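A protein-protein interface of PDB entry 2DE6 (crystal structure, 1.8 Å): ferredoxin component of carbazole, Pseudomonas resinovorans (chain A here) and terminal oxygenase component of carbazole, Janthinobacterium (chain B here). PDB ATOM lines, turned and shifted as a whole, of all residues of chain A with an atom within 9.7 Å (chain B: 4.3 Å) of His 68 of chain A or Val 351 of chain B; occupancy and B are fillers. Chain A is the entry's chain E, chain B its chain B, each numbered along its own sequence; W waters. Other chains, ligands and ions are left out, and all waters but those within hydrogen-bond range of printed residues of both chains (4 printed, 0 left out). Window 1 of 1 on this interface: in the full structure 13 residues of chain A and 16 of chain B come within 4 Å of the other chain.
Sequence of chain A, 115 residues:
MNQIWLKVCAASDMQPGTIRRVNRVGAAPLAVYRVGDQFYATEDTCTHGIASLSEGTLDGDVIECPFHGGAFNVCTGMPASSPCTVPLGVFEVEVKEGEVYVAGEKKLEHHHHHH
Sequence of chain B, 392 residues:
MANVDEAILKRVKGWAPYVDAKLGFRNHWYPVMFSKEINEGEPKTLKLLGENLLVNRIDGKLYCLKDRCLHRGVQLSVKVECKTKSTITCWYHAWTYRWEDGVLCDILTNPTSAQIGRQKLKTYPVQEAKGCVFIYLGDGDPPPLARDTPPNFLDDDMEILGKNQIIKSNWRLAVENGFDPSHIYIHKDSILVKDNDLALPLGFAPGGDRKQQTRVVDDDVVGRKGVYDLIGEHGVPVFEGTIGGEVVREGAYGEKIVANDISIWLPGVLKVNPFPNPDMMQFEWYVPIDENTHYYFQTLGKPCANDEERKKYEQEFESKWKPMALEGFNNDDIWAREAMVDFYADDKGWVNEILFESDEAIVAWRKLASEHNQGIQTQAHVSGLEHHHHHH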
ATOM      1  N   CYS A  46     -19.046  32.474  -3.856  1.00  0.00           N
ATOM      2  CA  CYS A  46     -17.688  32.744  -4.313  1.00  0.00           C
ATOM      3  C   CYS A  46     -17.667  34.129  -4.945  1.00  0.00           C
ATOM      4  O   CYS A  46     -18.548  34.461  -5.734  1.00  0.00           O
ATOM      5  CB  CYS A  46     -17.256  31.706  -5.351  1.00  0.00           C
ATOM      6  SG  CYS A  46     -15.561  31.941  -5.907  1.00  0.00           S
ATOM      7  N   THR A  47     -16.658  34.930  -4.614  1.00  0.00           N
ATOM      8  CA  THR A  47     -16.575  36.282  -5.160  1.00  0.00           C
ATOM      9  C   THR A  47     -16.257  36.309  -6.651  1.00  0.00           C
ATOM     10  O   THR A  47     -16.364  37.356  -7.290  1.00  0.00           O
ATOM     11  CB  THR A  47     -15.512  37.127  -4.422  1.00  0.00           C
ATOM     12  OG1 THR A  47     -14.205  36.617  -4.706  1.00  0.00           O
ATOM     13  CG2 THR A  47     -15.759  37.092  -2.915  1.00  0.00           C
ATOM     14  N   HIS A  48     -15.873  35.162  -7.204  1.00  0.00           N
ATOM     15  CA  HIS A  48     -15.547  35.082  -8.626  1.00  0.00           C
ATOM     16  C   HIS A  48     -16.757  34.738  -9.494  1.00  0.00           C
ATOM     17  O   HIS A  48     -16.689  34.795 -10.722  1.00  0.00           O
ATOM     18  CB  HIS A  48     -14.436  34.050  -8.846  1.00  0.00           C
ATOM     19  CG  HIS A  48     -14.038  33.883 -10.282  1.00  0.00           C
ATOM     20  ND1 HIS A  48     -14.401  32.784 -11.031  1.00  0.00           N
ATOM     21  CD2 HIS A  48     -13.314  34.676 -11.106  1.00  0.00           C
ATOM     22  CE1 HIS A  48     -13.917  32.908 -12.254  1.00  0.00           C
ATOM     23  NE2 HIS A  48     -13.254  34.049 -12.326  1.00  0.00           N
ATOM     24  N   GLY A  49     -17.871  34.384  -8.867  1.00  0.00           N
ATOM     25  CA  GLY A  49     -19.041  34.039  -9.652  1.00  0.00           C
ATOM     26  C   GLY A  49     -20.297  33.817  -8.841  1.00  0.00           C
ATOM     27  O   GLY A  49     -20.649  34.642  -8.000  1.00  0.00           O
ATOM     28  N   ILE A  50     -20.972  32.702  -9.102  1.00  0.00           N
ATOM     29  CA  ILE A  50     -22.213  32.366  -8.408  1.00  0.00           C
ATOM     30  C   ILE A  50     -22.143  31.018  -7.696  1.00  0.00           C
ATOM     31  O   ILE A  50     -23.165  30.476  -7.283  1.00  0.00           O
ATOM     32  CB  ILE A  50     -23.402  32.321  -9.388  1.00  0.00           C
ATOM     33  CG1 ILE A  50     -23.110  31.319 -10.507  1.00  0.00           C
ATOM     34  CG2 ILE A  50     -23.672  33.716  -9.954  1.00  0.00           C
ATOM     35  CD1 ILE A  50     -24.240  31.162 -11.501  1.00  0.00           C
ATOM     36  N   ALA A  51     -20.941  30.478  -7.546  1.00  0.00           N
ATOM     37  CA  ALA A  51     -20.777  29.190  -6.881  1.00  0.00           C
ATOM     38  C   ALA A  51     -20.987  29.277  -5.372  1.00  0.00           C
ATOM     39  O   ALA A  51     -20.812  30.334  -4.771  1.00  0.00           O
ATOM     40  CB  ALA A  51     -19.396  28.637  -7.169  1.00  0.00           C
ATOM     41  N   SER A  52     -21.365  28.152  -4.771  1.00  0.00           N
ATOM     42  CA  SER A  52     -21.565  28.075  -3.328  1.00  0.00           C
ATOM     43  C   SER A  52     -20.323  27.425  -2.719  1.00  0.00           C
ATOM     44  O   SER A  52     -20.030  26.257  -2.984  1.00  0.00           O
ATOM     45  CB  SER A  52     -22.804  27.237  -3.005  1.00  0.00           C
ATOM     46  OG  SER A  52     -22.913  27.017  -1.609  1.00  0.00           O
ATOM     47  N   LEU A  53     -19.592  28.185  -1.913  1.00  0.00           N
ATOM     48  CA  LEU A  53     -18.375  27.681  -1.287  1.00  0.00           C
ATOM     49  C   LEU A  53     -18.619  26.528  -0.320  1.00  0.00           C
ATOM     50  O   LEU A  53     -17.713  25.734  -0.065  1.00  0.00           O
ATOM     51  CB  LEU A  53     -17.639  28.815  -0.568  1.00  0.00           C
ATOM     52  CG  LEU A  53     -17.082  29.913  -1.477  1.00  0.00           C
ATOM     53  CD1 LEU A  53     -16.414  30.986  -0.633  1.00  0.00           C
ATOM     54  CD2 LEU A  53     -16.085  29.309  -2.462  1.00  0.00           C
ATOM     55  N   GLY A  56     -17.796  23.355  -1.783  1.00  0.00           N
ATOM     56  CA  GLY A  56     -16.416  23.160  -2.192  1.00  0.00           C
ATOM     57  C   GLY A  56     -15.643  22.223  -1.285  1.00  0.00           C
ATOM     58  O   GLY A  56     -16.231  21.423  -0.557  1.00  0.00           O
ATOM     59  N   ILE A  63     -10.420  27.224   1.555  1.00  0.00           N
ATOM     60  CA  ILE A  63     -11.606  26.678   0.904  1.00  0.00           C
ATOM     61  C   ILE A  63     -11.479  26.802  -0.617  1.00  0.00           C
ATOM     62  O   ILE A  63     -11.181  27.876  -1.138  1.00  0.00           O
ATOM     63  CB  ILE A  63     -12.888  27.416   1.379  1.00  0.00           C
ATOM     64  CG1 ILE A  63     -14.119  26.862   0.661  1.00  0.00           C
ATOM     65  CG2 ILE A  63     -12.752  28.913   1.136  1.00  0.00           C
ATOM     66  CD1 ILE A  63     -14.406  25.402   0.963  1.00  0.00           C
ATOM     67  N   GLU A  64     -11.700  25.694  -1.318  1.00  0.00           N
ATOM     68  CA  GLU A  64     -11.610  25.667  -2.776  1.00  0.00           C
ATOM     69  C   GLU A  64     -12.989  25.650  -3.436  1.00  0.00           C
ATOM     70  O   GLU A  64     -13.816  24.779  -3.154  1.00  0.00           O
ATOM     71  CB  GLU A  64     -10.815  24.437  -3.225  1.00  0.00           C
ATOM     72  CG  GLU A  64     -10.876  24.173  -4.723  1.00  0.00           C
ATOM     73  CD  GLU A  64     -10.226  22.856  -5.110  1.00  0.00           C
ATOM     74  OE1 GLU A  64      -8.986  22.820  -5.260  1.00  0.00           O
ATOM     75  OE2 GLU A  64     -10.959  21.853  -5.248  1.00  0.00           O
ATOM     76  N   CYS A  65     -13.225  26.611  -4.325  1.00  0.00           N
ATOM     77  CA  CYS A  65     -14.497  26.720  -5.034  1.00  0.00           C
ATOM     78  C   CYS A  65     -14.695  25.565  -6.016  1.00  0.00           C
ATOM     79  O   CYS A  65     -13.789  25.231  -6.777  1.00  0.00           O
ATOM     80  CB  CYS A  65     -14.558  28.045  -5.793  1.00  0.00           C
ATOM     81  SG  CYS A  65     -16.055  28.246  -6.769  1.00  0.00           S
ATOM     82  N   PRO A  66     -15.894  24.957  -6.023  1.00  0.00           N
ATOM     83  CA  PRO A  66     -16.216  23.833  -6.912  1.00  0.00           C
ATOM     84  C   PRO A  66     -16.435  24.174  -8.386  1.00  0.00           C
ATOM     85  O   PRO A  66     -16.503  23.274  -9.225  1.00  0.00           O
ATOM     86  CB  PRO A  66     -17.467  23.245  -6.273  1.00  0.00           C
ATOM     87  CG  PRO A  66     -18.165  24.469  -5.766  1.00  0.00           C
ATOM     88  CD  PRO A  66     -17.027  25.249  -5.125  1.00  0.00           C
ATOM     89  N   PHE A  67     -16.543  25.461  -8.705  1.00  0.00           N
ATOM     90  CA  PHE A  67     -16.772  25.878 -10.086  1.00  0.00           C
ATOM     91  C   PHE A  67     -15.517  26.028 -10.940  1.00  0.00           C
ATOM     92  O   PHE A  67     -15.420  25.416 -12.004  1.00  0.00           O
ATOM     93  CB  PHE A  67     -17.557  27.191 -10.122  1.00  0.00           C
ATOM     94  CG  PHE A  67     -19.051  27.012 -10.145  1.00  0.00           C
ATOM     95  CD1 PHE A  67     -19.649  25.896  -9.565  1.00  0.00           C
ATOM     96  CD2 PHE A  67     -19.867  27.983 -10.719  1.00  0.00           C
ATOM     97  CE1 PHE A  67     -21.040  25.751  -9.555  1.00  0.00           C
ATOM     98  CE2 PHE A  67     -21.256  27.851 -10.714  1.00  0.00           C
ATOM     99  CZ  PHE A  67     -21.842  26.731 -10.130  1.00  0.00           C
ATOM    100  N   HIS A  68     -14.560  26.834 -10.487  1.00  0.00           N
ATOM    101  CA  HIS A  68     -13.343  27.042 -11.271  1.00  0.00           C
ATOM    102  C   HIS A  68     -12.034  26.761 -10.541  1.00  0.00           C
ATOM    103  O   HIS A  68     -10.957  27.020 -11.076  1.00  0.00           O
ATOM    104  CB  HIS A  68     -13.315  28.471 -11.814  1.00  0.00           C
ATOM    105  CG  HIS A  68     -14.525  28.837 -12.612  1.00  0.00           C
ATOM    106  ND1 HIS A  68     -15.448  29.765 -12.178  1.00  0.00           N
ATOM    107  CD2 HIS A  68     -14.963  28.406 -13.818  1.00  0.00           C
ATOM    108  CE1 HIS A  68     -16.402  29.892 -13.083  1.00  0.00           C
ATOM    109  NE2 HIS A  68     -16.132  29.078 -14.089  1.00  0.00           N
ATOM    110  N   GLY A  69     -12.124  26.248  -9.319  1.00  0.00           N
ATOM    111  CA  GLY A  69     -10.920  25.938  -8.574  1.00  0.00           C
ATOM    112  C   GLY A  69     -10.256  27.099  -7.861  1.00  0.00           C
ATOM    113  O   GLY A  69      -9.131  26.963  -7.390  1.00  0.00           O
ATOM    114  N   GLY A  70     -10.930  28.244  -7.793  1.00  0.00           N
ATOM    115  CA  GLY A  70     -10.361  29.375  -7.082  1.00  0.00           C
ATOM    116  C   GLY A  70     -10.413  29.004  -5.610  1.00  0.00           C
ATOM    117  O   GLY A  70     -11.095  28.049  -5.253  1.00  0.00           O
ATOM    118  N   ALA A  71      -9.705  29.733  -4.753  1.00  0.00           N
ATOM    119  CA  ALA A  71      -9.716  29.408  -3.328  1.00  0.00           C
ATOM    120  C   ALA A  71      -9.508  30.627  -2.440  1.00  0.00           C
ATOM    121  O   ALA A  71      -8.990  31.647  -2.884  1.00  0.00           O
ATOM    122  CB  ALA A  71      -8.647  28.361  -3.022  1.00  0.00           C
ATOM    123  N   PHE A  72      -9.916  30.504  -1.180  1.00  0.00           N
ATOM    124  CA  PHE A  72      -9.768  31.587  -0.213  1.00  0.00           C
ATOM    125  C   PHE A  72      -9.302  31.031   1.122  1.00  0.00           C
ATOM    126  O   PHE A  72      -9.504  29.856   1.423  1.00  0.00           O
ATOM    127  CB  PHE A  72     -11.099  32.297   0.051  1.00  0.00           C
ATOM    128  CG  PHE A  72     -11.770  32.842  -1.172  1.00  0.00           C
ATOM    129  CD1 PHE A  72     -12.547  32.021  -1.979  1.00  0.00           C
ATOM    130  CD2 PHE A  72     -11.654  34.189  -1.498  1.00  0.00           C
ATOM    131  CE1 PHE A  72     -13.205  32.536  -3.093  1.00  0.00           C
ATOM    132  CE2 PHE A  72     -12.307  34.710  -2.609  1.00  0.00           C
ATOM    133  CZ  PHE A  72     -13.085  33.880  -3.407  1.00  0.00           C
ATOM    134  N   SER A  81      -6.066  31.121  -4.346  1.00  0.00           N
ATOM    135  CA  SER A  81      -5.795  30.566  -5.671  1.00  0.00           C
ATOM    136  C   SER A  81      -6.587  31.315  -6.729  1.00  0.00           C
ATOM    137  O   SER A  81      -7.710  31.751  -6.480  1.00  0.00           O
ATOM    138  CB  SER A  81      -6.185  29.084  -5.741  1.00  0.00           C
ATOM    139  OG  SER A  81      -5.388  28.277  -4.898  1.00  0.00           O
ATOM    140  N   SER A  82      -5.995  31.466  -7.907  1.00  0.00           N
ATOM    141  CA  SER A  82      -6.674  32.123  -9.015  1.00  0.00           C
ATOM    142  C   SER A  82      -7.833  31.195  -9.374  1.00  0.00           C
ATOM    143  O   SER A  82      -7.811  30.018  -9.020  1.00  0.00           O
ATOM    144  CB  SER A  82      -5.725  32.254 -10.207  1.00  0.00           C
ATOM    145  OG  SER A  82      -5.228  30.981 -10.592  1.00  0.00           O
ATOM    146  N   PRO A  83      -8.846  31.696 -10.099  1.00  0.00           N
ATOM    147  CA  PRO A  83      -8.998  33.058 -10.622  1.00  0.00           C
ATOM    148  C   PRO A  83      -9.557  34.073  -9.623  1.00  0.00           C
ATOM    149  O   PRO A  83      -9.809  35.223  -9.979  1.00  0.00           O
ATOM    150  CB  PRO A  83      -9.930  32.855 -11.808  1.00  0.00           C
ATOM    151  CG  PRO A  83     -10.857  31.789 -11.293  1.00  0.00           C
ATOM    152  CD  PRO A  83      -9.919  30.818 -10.606  1.00  0.00           C
ATOM    153  N   CYS A  84      -9.766  33.653  -8.380  1.00  0.00           N
ATOM    154  CA  CYS A  84     -10.293  34.567  -7.371  1.00  0.00           C
ATOM    155  C   CYS A  84      -9.347  35.733  -7.098  1.00  0.00           C
ATOM    156  O   CYS A  84      -8.134  35.547  -6.976  1.00  0.00           O
ATOM    157  CB  CYS A  84     -10.579  33.807  -6.078  1.00  0.00           C
ATOM    158  SG  CYS A  84     -11.902  32.600  -6.284  1.00  0.00           S
ATOM    159  N   ILE B   8      -6.837  22.142 -16.377  1.00  0.00           N
ATOM    160  CA  ILE B   8      -8.071  22.905 -16.520  1.00  0.00           C
ATOM    161  C   ILE B   8      -9.265  22.036 -16.148  1.00  0.00           C
ATOM    162  O   ILE B   8     -10.158  22.469 -15.423  1.00  0.00           O
ATOM    163  CB  ILE B   8      -8.242  23.427 -17.968  1.00  0.00           C
ATOM    164  CG1 ILE B   8      -7.146  24.449 -18.283  1.00  0.00           C
ATOM    165  CG2 ILE B   8      -9.623  24.056 -18.141  1.00  0.00           C
ATOM    166  CD1 ILE B   8      -7.164  24.964 -19.714  1.00  0.00           C
ATOM    167  N   ARG B  11      -9.942  21.686 -12.548  1.00  0.00           N
ATOM    168  CA  ARG B  11     -10.515  22.889 -11.950  1.00  0.00           C
ATOM    169  C   ARG B  11     -12.030  22.997 -12.105  1.00  0.00           C
ATOM    170  O   ARG B  11     -12.718  23.392 -11.167  1.00  0.00           O
ATOM    171  CB  ARG B  11      -9.862  24.141 -12.549  1.00  0.00           C
ATOM    172  CG  ARG B  11      -8.552  24.560 -11.892  1.00  0.00           C
ATOM    173  CD  ARG B  11      -7.965  25.765 -12.612  1.00  0.00           C
ATOM    174  NE  ARG B  11      -6.869  26.397 -11.880  1.00  0.00           N
ATOM    175  CZ  ARG B  11      -7.034  27.266 -10.884  1.00  0.00           C
ATOM    176  NH1 ARG B  11      -8.254  27.615 -10.497  1.00  0.00           N
ATOM    177  NH2 ARG B  11      -5.977  27.793 -10.282  1.00  0.00           N
ATOM    178  N   TRP B  15     -18.503  20.546 -14.400  1.00  0.00           N
ATOM    179  CA  TRP B  15     -18.856  20.166 -15.766  1.00  0.00           C
ATOM    180  C   TRP B  15     -17.631  19.883 -16.634  1.00  0.00           C
ATOM    181  O   TRP B  15     -17.524  20.368 -17.766  1.00  0.00           O
ATOM    182  CB  TRP B  15     -19.713  21.275 -16.390  1.00  0.00           C
ATOM    183  CG  TRP B  15     -19.143  22.660 -16.204  1.00  0.00           C
ATOM    184  CD1 TRP B  15     -18.174  23.254 -16.957  1.00  0.00           C
ATOM    185  CD2 TRP B  15     -19.503  23.612 -15.190  1.00  0.00           C
ATOM    186  NE1 TRP B  15     -17.907  24.518 -16.481  1.00  0.00           N
ATOM    187  CE2 TRP B  15     -18.708  24.762 -15.396  1.00  0.00           C
ATOM    188  CE3 TRP B  15     -20.417  23.604 -14.127  1.00  0.00           C
ATOM    189  CZ2 TRP B  15     -18.799  25.898 -14.578  1.00  0.00           C
ATOM    190  CZ3 TRP B  15     -20.508  24.734 -13.313  1.00  0.00           C
ATOM    191  CH2 TRP B  15     -19.703  25.863 -13.545  1.00  0.00           C
ATOM    192  N   LYS B 348      -8.820  28.743 -21.542  1.00  0.00           N
ATOM    193  CA  LYS B 348      -8.749  29.495 -20.289  1.00  0.00           C
ATOM    194  C   LYS B 348     -10.039  30.204 -19.872  1.00  0.00           C
ATOM    195  O   LYS B 348     -10.258  30.454 -18.687  1.00  0.00           O
ATOM    196  CB  LYS B 348      -7.602  30.507 -20.357  1.00  0.00           C
ATOM    197  CG  LYS B 348      -6.232  29.877 -20.602  1.00  0.00           C
ATOM    198  CD  LYS B 348      -5.874  28.872 -19.521  1.00  0.00           C
ATOM    199  CE  LYS B 348      -4.507  28.235 -19.772  1.00  0.00           C
ATOM    200  NZ  LYS B 348      -3.389  29.218 -19.717  1.00  0.00           N
ATOM    201  N   GLY B 349     -10.886  30.531 -20.842  1.00  0.00           N
ATOM    202  CA  GLY B 349     -12.138  31.195 -20.524  1.00  0.00           C
ATOM    203  C   GLY B 349     -13.018  30.333 -19.633  1.00  0.00           C
ATOM    204  O   GLY B 349     -13.826  30.852 -18.858  1.00  0.00           O
ATOM    205  N   TRP B 350     -12.866  29.016 -19.745  1.00  0.00           N
ATOM    206  CA  TRP B 350     -13.650  28.084 -18.941  1.00  0.00           C
ATOM    207  C   TRP B 350     -13.284  28.190 -17.463  1.00  0.00           C
ATOM    208  O   TRP B 350     -13.967  27.634 -16.599  1.00  0.00           O
ATOM    209  CB  TRP B 350     -13.437  26.643 -19.426  1.00  0.00           C
ATOM    210  CG  TRP B 350     -13.893  26.415 -20.835  1.00  0.00           C
ATOM    211  CD1 TRP B 350     -13.103  26.176 -21.926  1.00  0.00           C
ATOM    212  CD2 TRP B 350     -15.243  26.437 -21.314  1.00  0.00           C
ATOM    213  NE1 TRP B 350     -13.878  26.049 -23.054  1.00  0.00           N
ATOM    214  CE2 TRP B 350     -15.195  26.206 -22.708  1.00  0.00           C
ATOM    215  CE3 TRP B 350     -16.489  26.632 -20.701  1.00  0.00           C
ATOM    216  CZ2 TRP B 350     -16.347  26.166 -23.501  1.00  0.00           C
ATOM    217  CZ3 TRP B 350     -17.636  26.594 -21.489  1.00  0.00           C
ATOM    218  CH2 TRP B 350     -17.555  26.363 -22.876  1.00  0.00           C
ATOM    219  N   VAL B 351     -12.203  28.902 -17.174  1.00  0.00           N
ATOM    220  CA  VAL B 351     -11.768  29.081 -15.795  1.00  0.00           C
ATOM    221  C   VAL B 351     -11.911  30.531 -15.338  1.00  0.00           C
ATOM    222  O   VAL B 351     -12.291  30.792 -14.199  1.00  0.00           O
ATOM    223  CB  VAL B 351     -10.283  28.675 -15.613  1.00  0.00           C
ATOM    224  CG1 VAL B 351      -9.815  29.021 -14.200  1.00  0.00           C
ATOM    225  CG2 VAL B 351     -10.112  27.185 -15.867  1.00  0.00           C
ATOM    226  N   ASN B 352     -11.626  31.466 -16.238  1.00  0.00           N
ATOM    227  CA  ASN B 352     -11.659  32.888 -15.903  1.00  0.00           C
ATOM    228  C   ASN B 352     -12.977  33.653 -16.022  1.00  0.00           C
ATOM    229  O   ASN B 352     -13.076  34.782 -15.541  1.00  0.00           O
ATOM    230  CB  ASN B 352     -10.571  33.612 -16.703  1.00  0.00           C
ATOM    231  CG  ASN B 352      -9.175  33.163 -16.317  1.00  0.00           C
ATOM    232  OD1 ASN B 352      -8.839  33.104 -15.135  1.00  0.00           O
ATOM    233  ND2 ASN B 352      -8.351  32.852 -17.310  1.00  0.00           N
ATOM    234  N   GLU B 353     -13.976  33.052 -16.658  1.00  0.00           N
ATOM    235  CA  GLU B 353     -15.282  33.688 -16.820  1.00  0.00           C
ATOM    236  C   GLU B 353     -15.860  34.074 -15.454  1.00  0.00           C
ATOM    237  O   GLU B 353     -15.751  33.314 -14.497  1.00  0.00           O
ATOM    238  CB  GLU B 353     -16.244  32.708 -17.499  1.00  0.00           C
ATOM    239  CG  GLU B 353     -16.324  31.388 -16.736  1.00  0.00           C
ATOM    240  CD  GLU B 353     -17.237  30.350 -17.369  1.00  0.00           C
ATOM    241  OE1 GLU B 353     -17.623  30.507 -18.546  1.00  0.00           O
ATOM    242  OE2 GLU B 353     -17.554  29.358 -16.677  1.00  0.00           O
HETATM  243  O   HOH W   1      -6.561  29.970 -12.582  1.00  0.00           O
HETATM  244  O   HOH W   2     -17.513  32.841 -12.483  1.00  0.00           O
HETATM  245  O   HOH W   3     -11.103  36.186 -13.364  1.00  0.00           O
HETATM  246  O   HOH W   4     -12.580  23.079  -8.114  1.00  0.00           O
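The backbone carbonyl oxygen (O) of Glu 353 of chain B lies close to a ring nitrogen (NE2) of His 48 of chain A (3.4 Å). OE2 of Glu 353 of chain B sits at hydrogen-bond distance from NE2 of His 68 of chain A, 3.0 Å away. O of His 68 of chain A sits at hydrogen-bond distance from NH1 of Arg 11 of chain B (2.8 Å). The backbone carbonyl oxygen (O) of Phe 67 of chain A sits close to the backbone carbonyl oxygen (O) of Arg 11 of chain B, 3.5 Å away. The guanidinium group (NH1) of Arg 11 of chain B sits at hydrogen-bond distance from the backbone carbonyl oxygen (O) of Gly 69 of chain A (3.3 Å). The backbone carbonyl oxygen (O) of Asn 352 of chain B is in hydrogen-bond range of a ring nitrogen (NE2) of His 48 of chain A (3.3 Å). The guanidinium group (NH1) of Arg 11 of chain B sits at hydrogen-bond distance from the backbone carbonyl oxygen (O) of Ser 82 of chain A.
ND2 of Asn 352 of chain B lies within hydrogen-bond range of O of Lys 348 of chain B (3.4 Å). The side-chain sulfur of Cys 65 of chain A lies close to the backbone NH of Phe 67 of chain A (3.4 Å). The backbone NH (N) of His 48 of chain A sits close to the side-chain sulfur (SG) of Cys 46 of chain A. N of Cys 65 of chain A lies within hydrogen-bond range of O of Gly 70 of chain A (2.7 Å).
Water W1 bridges OG of Ser 82 of chain A (2.6 Å) and NH2 of Arg 11 of chain B (3.2 Å). Water W2 lies within hydrogen-bond range of the backbone carbonyl oxygen (O) of Glu 353 of chain B (2.7 Å) and the backbone carbonyl oxygen (O) of His 48 of chain A (2.8 Å). Water W4 lies within hydrogen-bond range of the backbone carbonyl oxygen (O) of Cys 65 of chain A (2.8 Å), the backbone carbonyl oxygen (O) of Arg 11 of chain B (3.1 Å) and the backbone NH (N) of Gly 69 of chain A (3.4 Å). Water W3 lies within hydrogen-bond range of NE2 of His 48 of chain A (3.2 Å) and O of Asn 352 of chain B (3.3 Å).
Of the printed residues of chain B, His 48 of chain A touches Val 351 (3.3 Å), Asn 352 (3.3 Å) and Glu 353 (2.9 Å). Ile 50 of chain A touches none of the printed residues of chain B. Ala 51 of chain A touches none of the printed residues of chain B. His 68 of chain A touches just these residues of chain B: Arg 11, Trp 350, Val 351 and Glu 353. Of the printed residues of chain B, Gly 69 of chain A touches Arg 11 (3.3 Å). Printed residues of chain B within 4 Å of Gly 70 of chain A: Arg 11 (3.9 Å). Of the printed residues of chain A, Trp 15 of chain B touches Phe 67 (3.5 Å). Val 351 of chain B touches just these residues of chain A: His 48, His 68 and Pro 83. The nearest residue of chain A that does not touch Val 351 of chain B is Ser 82 of chain A (5.6 Å). The nearest printed residue of chain B that does not touch Gly 70 of chain A is Val 351 of chain B (6.5 Å).
Of the 9 printed residues of chain B, 6 touch a printed residue of chain A. Hydrophobic or aromatic side chains of chain B that line the printed part of chain A: Trp 15 and Val 351. Of the 23 printed residues of chain A, 7 touch a printed residue of chain B. Printed residues of chain A that touch a printed residue of chain B: His 48, Phe 67, His 68, Gly 69, Gly 70, Ser 82 and Pro 83. Among the printed residues, 15 pairs touch across the chains. Among the printed residues, no Asp or Glu carboxylate lies within 4 Å of a Lys or Arg side-chain nitrogen of the other chain.
Among the printed residues, merely in contact across the chains: His 68 of chain A with Trp 350 of chain B (3.1 Å), His 48 of chain A with Val 351 of chain B (3.3 Å), His 68 of chain A with Val 351 of chain B (3.4 Å), Pro 83 of chain A with Val 351 of chain B (3.4 Å), Pro 83 of chain A with Asn 352 of chain B (3.5 Å), Phe 67 of chain A with Trp 15 of chain B (3.5 Å), Pro 83 of chain A with Arg 11 of chain B (3.6 Å) and Gly 70 of chain A with Arg 11 of chain B (3.9 Å).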
